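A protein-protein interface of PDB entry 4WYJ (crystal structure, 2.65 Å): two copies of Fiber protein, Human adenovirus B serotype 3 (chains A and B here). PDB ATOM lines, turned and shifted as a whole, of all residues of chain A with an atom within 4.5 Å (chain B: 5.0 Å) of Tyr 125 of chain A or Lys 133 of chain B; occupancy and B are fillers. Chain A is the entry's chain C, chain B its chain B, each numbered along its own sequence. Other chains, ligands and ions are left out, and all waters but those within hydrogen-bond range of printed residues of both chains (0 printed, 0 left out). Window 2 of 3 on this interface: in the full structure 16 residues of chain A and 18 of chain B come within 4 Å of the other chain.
The backbone NH (N) of Ser 183 of chain B sits at hydrogen-bond distance from the backbone carbonyl oxygen (O) of Tyr 131 of chain B, 2.8 Å away.
N of Val 146 of chain A lies within hydrogen-bond range of O of Ile 126 of chain A, at 2.8 Å.
Among the printed residues, pairs that only touch across the chains: Asn 122 of chain A with Ile 181 of chain B, Glu 123 of chain A with Ile 181 of chain B, Tyr 125 of chain A with Lys 133 of chain B, Tyr 125 of chain A with Ser 183 of chain B, Tyr 125 of chain A with Pro 184 of chain B, Ile 126 of chain A with Pro 184 of chain B, Phe 127 of chain A with Tyr 131 of chain B, Phe 127 of chain A with Leu 139 of chain B and Phe 127 of chain A with Ser 183 of chain B.
Printed residues of chain B within 4 Å of Asn 122 of chain A: Ile 181 (3.9 Å).
Printed residues of chain B within 4 Å of Glu 123 of chain A: Ile 181.
Tyr 125 of chain A touches three residues of chain B.
Of the printed residues of chain A, Tyr 131 of chain B touches Phe 127 (3.4 Å).
Of the printed residues of chain A, Lys 133 of chain B touches Tyr 125.
The nearest printed residue of chain B that does not touch Ile 126 of chain A is Ser 183 of chain B (4.9 Å).
Printed residues of chain B that touch a printed residue of chain A: Tyr 131, Lys 133, Leu 139, Ile 181, Ser 183 and Pro 184.
Hydrophobic or aromatic side chains of chain B within 4 Å of the printed part of chain A: Tyr 131, Leu 139, Ile 181 and Pro 184.
Of the 10 printed residues of chain A, 5 touch a printed residue of chain B.
Printed residues of chain A that touch a printed residue of chain B: Asn 122, Glu 123, Tyr 125, Ile 126 and Phe 127.
Hydrophobic or aromatic side chains of chain A within 4 Å of the printed part of chain B: Tyr 125, Ile 126 and Phe 127.
Along chain A the printed residues that touch a printed residue of chain B span positions 122 to 127.
Among the printed residues, 9 pairs touch across the chains.
Among the printed residues, no Asp or Glu carboxylate lies within 4 Å of a Lys or Arg side-chain nitrogen of the other chain.
No position is printed for both chains.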
ATOM      1  N   ASN A 122     -16.557  10.827 -29.496  1.00  0.00           N
ATOM      2  CA  ASN A 122     -15.207  10.786 -28.915  1.00  0.00           C
ATOM      3  C   ASN A 122     -14.561  12.170 -28.837  1.00  0.00           C
ATOM      4  O   ASN A 122     -13.491  12.306 -28.271  1.00  0.00           O
ATOM      5  CB  ASN A 122     -14.321   9.763 -29.615  1.00  0.00           C
ATOM      6  CG  ASN A 122     -14.498   8.343 -29.135  1.00  0.00           C
ATOM      7  OD1 ASN A 122     -15.259   8.026 -28.207  1.00  0.00           O
ATOM      8  ND2 ASN A 122     -13.742   7.456 -29.735  1.00  0.00           N
ATOM      9  N   GLU A 123     -15.270  13.201 -29.293  1.00  0.00           N
ATOM     10  CA  GLU A 123     -14.865  14.600 -29.227  1.00  0.00           C
ATOM     11  C   GLU A 123     -15.155  15.176 -27.850  1.00  0.00           C
ATOM     12  O   GLU A 123     -14.826  16.337 -27.608  1.00  0.00           O
ATOM     13  CB  GLU A 123     -15.572  15.433 -30.312  1.00  0.00           C
ATOM     14  CG  GLU A 123     -17.091  15.418 -30.253  1.00  0.00           C
ATOM     15  CD  GLU A 123     -17.752  14.414 -31.170  1.00  0.00           C
ATOM     16  OE1 GLU A 123     -17.146  13.351 -31.431  1.00  0.00           O
ATOM     17  OE2 GLU A 123     -18.882  14.688 -31.634  1.00  0.00           O
ATOM     18  N   ASN A 124     -15.793  14.374 -26.966  1.00  0.00           N
ATOM     19  CA  ASN A 124     -16.228  14.722 -25.612  1.00  0.00           C
ATOM     20  C   ASN A 124     -15.182  14.461 -24.556  1.00  0.00           C
ATOM     21  O   ASN A 124     -15.429  14.734 -23.364  1.00  0.00           O
ATOM     22  CB  ASN A 124     -17.496  13.944 -25.253  1.00  0.00           C
ATOM     23  CG  ASN A 124     -18.727  14.394 -25.979  1.00  0.00           C
ATOM     24  OD1 ASN A 124     -18.660  14.828 -27.133  1.00  0.00           O
ATOM     25  ND2 ASN A 124     -19.892  14.210 -25.352  1.00  0.00           N
ATOM     26  N   TYR A 125     -14.012  13.944 -24.975  1.00  0.00           N
ATOM     27  CA  TYR A 125     -12.904  13.645 -24.074  1.00  0.00           C
ATOM     28  C   TYR A 125     -11.788  14.642 -24.147  1.00  0.00           C
ATOM     29  O   TYR A 125     -11.350  14.991 -25.234  1.00  0.00           O
ATOM     30  CB  TYR A 125     -12.304  12.282 -24.409  1.00  0.00           C
ATOM     31  CG  TYR A 125     -13.242  11.120 -24.234  1.00  0.00           C
ATOM     32  CD1 TYR A 125     -13.632  10.701 -22.967  1.00  0.00           C
ATOM     33  CD2 TYR A 125     -13.706  10.407 -25.333  1.00  0.00           C
ATOM     34  CE1 TYR A 125     -14.475   9.613 -22.795  1.00  0.00           C
ATOM     35  CE2 TYR A 125     -14.532   9.300 -25.171  1.00  0.00           C
ATOM     36  CZ  TYR A 125     -14.918   8.910 -23.895  1.00  0.00           C
ATOM     37  OH  TYR A 125     -15.743   7.828 -23.696  1.00  0.00           O
ATOM     38  N   ILE A 126     -11.254  15.013 -22.991  1.00  0.00           N
ATOM     39  CA  ILE A 126     -10.055  15.844 -22.847  1.00  0.00           C
ATOM     40  C   ILE A 126      -9.064  14.939 -22.133  1.00  0.00           C
ATOM     41  O   ILE A 126      -9.405  14.353 -21.103  1.00  0.00           O
ATOM     42  CB  ILE A 126     -10.314  17.165 -22.064  1.00  0.00           C
ATOM     43  CG1 ILE A 126     -11.360  18.079 -22.787  1.00  0.00           C
ATOM     44  CG2 ILE A 126      -9.005  17.906 -21.808  1.00  0.00           C
ATOM     45  CD1 ILE A 126     -12.004  19.172 -21.896  1.00  0.00           C
ATOM     46  N   PHE A 127      -7.869  14.750 -22.723  1.00  0.00           N
ATOM     47  CA  PHE A 127      -6.812  13.926 -22.116  1.00  0.00           C
ATOM     48  C   PHE A 127      -5.625  14.803 -21.786  1.00  0.00           C
ATOM     49  O   PHE A 127      -5.309  15.716 -22.529  1.00  0.00           O
ATOM     50  CB  PHE A 127      -6.357  12.803 -23.049  1.00  0.00           C
ATOM     51  CG  PHE A 127      -7.463  11.941 -23.572  1.00  0.00           C
ATOM     52  CD1 PHE A 127      -8.036  10.945 -22.770  1.00  0.00           C
ATOM     53  CD2 PHE A 127      -7.947  12.120 -24.859  1.00  0.00           C
ATOM     54  CE1 PHE A 127      -9.064  10.157 -23.254  1.00  0.00           C
ATOM     55  CE2 PHE A 127      -8.967  11.325 -25.345  1.00  0.00           C
ATOM     56  CZ  PHE A 127      -9.527  10.355 -24.539  1.00  0.00           C
ATOM     57  N   THR A 145      -8.271  11.764 -17.783  1.00  0.00           N
ATOM     58  CA  THR A 145      -9.369  11.773 -18.754  1.00  0.00           C
ATOM     59  C   THR A 145     -10.540  12.567 -18.182  1.00  0.00           C
ATOM     60  O   THR A 145     -11.003  12.278 -17.078  1.00  0.00           O
ATOM     61  CB  THR A 145      -9.881  10.369 -19.114  1.00  0.00           C
ATOM     62  OG1 THR A 145      -8.800   9.512 -19.508  1.00  0.00           O
ATOM     63  CG2 THR A 145     -10.958  10.423 -20.214  1.00  0.00           C
ATOM     64  N   VAL A 146     -11.022  13.543 -18.946  1.00  0.00           N
ATOM     65  CA  VAL A 146     -12.213  14.332 -18.616  1.00  0.00           C
ATOM     66  C   VAL A 146     -13.278  13.954 -19.672  1.00  0.00           C
ATOM     67  O   VAL A 146     -12.989  13.953 -20.870  1.00  0.00           O
ATOM     68  CB  VAL A 146     -12.005  15.882 -18.517  1.00  0.00           C
ATOM     69  CG1 VAL A 146     -13.248  16.561 -17.941  1.00  0.00           C
ATOM     70  CG2 VAL A 146     -10.782  16.237 -17.687  1.00  0.00           C
ATOM     71  N   MET A 147     -14.464  13.557 -19.221  1.00  0.00           N
ATOM     72  CA  MET A 147     -15.554  13.249 -20.135  1.00  0.00           C
ATOM     73  C   MET A 147     -16.607  14.266 -19.889  1.00  0.00           C
ATOM     74  O   MET A 147     -16.971  14.517 -18.740  1.00  0.00           O
ATOM     75  CB  MET A 147     -16.107  11.848 -19.945  1.00  0.00           C
ATOM     76  CG  MET A 147     -17.096  11.433 -21.014  1.00  0.00           C
ATOM     77  SD  MET A 147     -17.923   9.941 -20.441  1.00  0.00           S
ATOM     78  CE  MET A 147     -19.233  10.686 -19.514  1.00  0.00           C
ATOM     79  N   LYS A 150     -21.879  13.187 -23.186  1.00  0.00           N
ATOM     80  CA  LYS A 150     -21.765  11.846 -23.803  1.00  0.00           C
ATOM     81  C   LYS A 150     -22.827  10.818 -23.330  1.00  0.00           C
ATOM     82  O   LYS A 150     -23.462  10.201 -24.189  1.00  0.00           O
ATOM     83  CB  LYS A 150     -20.336  11.282 -23.646  1.00  0.00           C
ATOM     84  CG  LYS A 150     -20.033  10.094 -24.531  1.00  0.00           C
ATOM     85  CD  LYS A 150     -18.605   9.636 -24.386  1.00  0.00           C
ATOM     86  CE  LYS A 150     -18.187   8.859 -25.601  1.00  0.00           C
ATOM     87  NZ  LYS A 150     -18.884   7.557 -25.677  1.00  0.00           N
ATOM     88  N   TYR B 131      -4.203  13.875 -27.736  1.00  0.00           N
ATOM     89  CA  TYR B 131      -4.305  12.421 -27.931  1.00  0.00           C
ATOM     90  C   TYR B 131      -5.308  12.032 -28.969  1.00  0.00           C
ATOM     91  O   TYR B 131      -6.226  12.803 -29.275  1.00  0.00           O
ATOM     92  CB  TYR B 131      -4.657  11.710 -26.575  1.00  0.00           C
ATOM     93  CG  TYR B 131      -3.639  11.967 -25.486  1.00  0.00           C
ATOM     94  CD1 TYR B 131      -3.543  13.220 -24.870  1.00  0.00           C
ATOM     95  CD2 TYR B 131      -2.724  10.982 -25.112  1.00  0.00           C
ATOM     96  CE1 TYR B 131      -2.544  13.498 -23.941  1.00  0.00           C
ATOM     97  CE2 TYR B 131      -1.745  11.236 -24.147  1.00  0.00           C
ATOM     98  CZ  TYR B 131      -1.659  12.499 -23.569  1.00  0.00           C
ATOM     99  OH  TYR B 131      -0.703  12.794 -22.626  1.00  0.00           O
ATOM    100  N   TYR B 132      -5.156  10.796 -29.476  1.00  0.00           N
ATOM    101  CA  TYR B 132      -6.104  10.136 -30.357  1.00  0.00           C
ATOM    102  C   TYR B 132      -6.586   8.882 -29.633  1.00  0.00           C
ATOM    103  O   TYR B 132      -5.766   8.021 -29.291  1.00  0.00           O
ATOM    104  CB  TYR B 132      -5.480   9.766 -31.714  1.00  0.00           C
ATOM    105  CG  TYR B 132      -6.424   8.954 -32.582  1.00  0.00           C
ATOM    106  CD1 TYR B 132      -7.584   9.524 -33.113  1.00  0.00           C
ATOM    107  CD2 TYR B 132      -6.168   7.614 -32.862  1.00  0.00           C
ATOM    108  CE1 TYR B 132      -8.460   8.776 -33.903  1.00  0.00           C
ATOM    109  CE2 TYR B 132      -7.042   6.856 -33.640  1.00  0.00           C
ATOM    110  CZ  TYR B 132      -8.189   7.440 -34.159  1.00  0.00           C
ATOM    111  OH  TYR B 132      -9.027   6.718 -34.974  1.00  0.00           O
ATOM    112  N   LYS B 133      -7.899   8.782 -29.381  1.00  0.00           N
ATOM    113  CA  LYS B 133      -8.494   7.589 -28.765  1.00  0.00           C
ATOM    114  C   LYS B 133      -8.928   6.691 -29.917  1.00  0.00           C
ATOM    115  O   LYS B 133      -9.862   7.037 -30.652  1.00  0.00           O
ATOM    116  CB  LYS B 133      -9.694   7.925 -27.833  1.00  0.00           C
ATOM    117  CG  LYS B 133     -10.194   6.710 -27.046  1.00  0.00           C
ATOM    118  CD  LYS B 133     -11.508   6.957 -26.376  1.00  0.00           C
ATOM    119  CE  LYS B 133     -11.901   5.808 -25.486  1.00  0.00           C
ATOM    120  NZ  LYS B 133     -13.380   5.757 -25.285  1.00  0.00           N
ATOM    121  N   ALA B 134      -8.223   5.553 -30.087  1.00  0.00           N
ATOM    122  CA  ALA B 134      -8.430   4.590 -31.168  1.00  0.00           C
ATOM    123  C   ALA B 134      -9.731   3.838 -30.990  1.00  0.00           C
ATOM    124  O   ALA B 134     -10.248   3.760 -29.867  1.00  0.00           O
ATOM    125  CB  ALA B 134      -7.250   3.636 -31.248  1.00  0.00           C
ATOM    126  N   SER B 135     -10.282   3.295 -32.091  1.00  0.00           N
ATOM    127  CA  SER B 135     -11.549   2.564 -32.066  1.00  0.00           C
ATOM    128  C   SER B 135     -11.605   1.436 -31.017  1.00  0.00           C
ATOM    129  O   SER B 135     -12.689   1.141 -30.506  1.00  0.00           O
ATOM    130  CB  SER B 135     -11.886   2.028 -33.451  1.00  0.00           C
ATOM    131  OG  SER B 135     -10.957   1.034 -33.845  1.00  0.00           O
ATOM    132  N   GLY B 137     -10.037   1.627 -28.107  1.00  0.00           N
ATOM    133  CA  GLY B 137      -9.902   2.268 -26.809  1.00  0.00           C
ATOM    134  C   GLY B 137      -8.490   2.639 -26.404  1.00  0.00           C
ATOM    135  O   GLY B 137      -8.312   3.296 -25.376  1.00  0.00           O
ATOM    136  N   ALA B 138      -7.471   2.244 -27.203  1.00  0.00           N
ATOM    137  CA  ALA B 138      -6.068   2.579 -26.945  1.00  0.00           C
ATOM    138  C   ALA B 138      -5.832   4.077 -27.152  1.00  0.00           C
ATOM    139  O   ALA B 138      -6.391   4.684 -28.069  1.00  0.00           O
ATOM    140  CB  ALA B 138      -5.156   1.769 -27.848  1.00  0.00           C
ATOM    141  N   LEU B 139      -5.033   4.671 -26.271  1.00  0.00           N
ATOM    142  CA  LEU B 139      -4.736   6.093 -26.296  1.00  0.00           C
ATOM    143  C   LEU B 139      -3.367   6.388 -26.832  1.00  0.00           C
ATOM    144  O   LEU B 139      -2.379   5.997 -26.222  1.00  0.00           O
ATOM    145  CB  LEU B 139      -4.896   6.685 -24.900  1.00  0.00           C
ATOM    146  CG  LEU B 139      -5.504   8.048 -24.872  1.00  0.00           C
ATOM    147  CD1 LEU B 139      -7.012   7.954 -25.137  1.00  0.00           C
ATOM    148  CD2 LEU B 139      -5.190   8.727 -23.568  1.00  0.00           C
ATOM    149  N   GLU B 174      -5.102   2.137 -35.999  1.00  0.00           N
ATOM    150  CA  GLU B 174      -6.222   1.507 -36.698  1.00  0.00           C
ATOM    151  C   GLU B 174      -5.820   0.531 -37.803  1.00  0.00           C
ATOM    152  O   GLU B 174      -4.721   0.631 -38.361  1.00  0.00           O
ATOM    153  CB  GLU B 174      -7.135   2.596 -37.327  1.00  0.00           C
ATOM    154  CG  GLU B 174      -7.661   3.676 -36.392  1.00  0.00           C
ATOM    155  CD  GLU B 174      -8.657   3.252 -35.333  1.00  0.00           C
ATOM    156  OE1 GLU B 174      -9.130   2.094 -35.374  1.00  0.00           O
ATOM    157  OE2 GLU B 174      -8.959   4.081 -34.451  1.00  0.00           O
ATOM    158  N   ILE B 181     -10.051  12.219 -34.729  1.00  0.00           N
ATOM    159  CA  ILE B 181     -10.376  13.253 -33.748  1.00  0.00           C
ATOM    160  C   ILE B 181      -9.127  13.466 -32.924  1.00  0.00           C
ATOM    161  O   ILE B 181      -8.651  12.509 -32.300  1.00  0.00           O
ATOM    162  CB  ILE B 181     -11.601  12.905 -32.812  1.00  0.00           C
ATOM    163  CG1 ILE B 181     -12.891  12.608 -33.603  1.00  0.00           C
ATOM    164  CG2 ILE B 181     -11.841  14.008 -31.732  1.00  0.00           C
ATOM    165  CD1 ILE B 181     -13.942  11.870 -32.822  1.00  0.00           C
ATOM    166  N   SER B 183      -7.791  15.136 -29.564  1.00  0.00           N
ATOM    167  CA  SER B 183      -8.370  15.680 -28.329  1.00  0.00           C
ATOM    168  C   SER B 183      -8.054  17.197 -28.169  1.00  0.00           C
ATOM    169  O   SER B 183      -7.073  17.671 -28.763  1.00  0.00           O
ATOM    170  CB  SER B 183      -7.967  14.843 -27.113  1.00  0.00           C
ATOM    171  OG  SER B 183      -6.651  15.068 -26.648  1.00  0.00           O
ATOM    172  N   PRO B 184      -8.882  17.994 -27.442  1.00  0.00           N
ATOM    173  CA  PRO B 184      -8.603  19.440 -27.359  1.00  0.00           C
ATOM    174  C   PRO B 184      -7.201  19.791 -26.870  1.00  0.00           C
ATOM    175  O   PRO B 184      -6.731  19.227 -25.887  1.00  0.00           O
ATOM    176  CB  PRO B 184      -9.691  19.948 -26.401  1.00  0.00           C
ATOM    177  CG  PRO B 184     -10.780  18.984 -26.525  1.00  0.00           C
ATOM    178  CD  PRO B 184     -10.090  17.657 -26.655  1.00  0.00           C
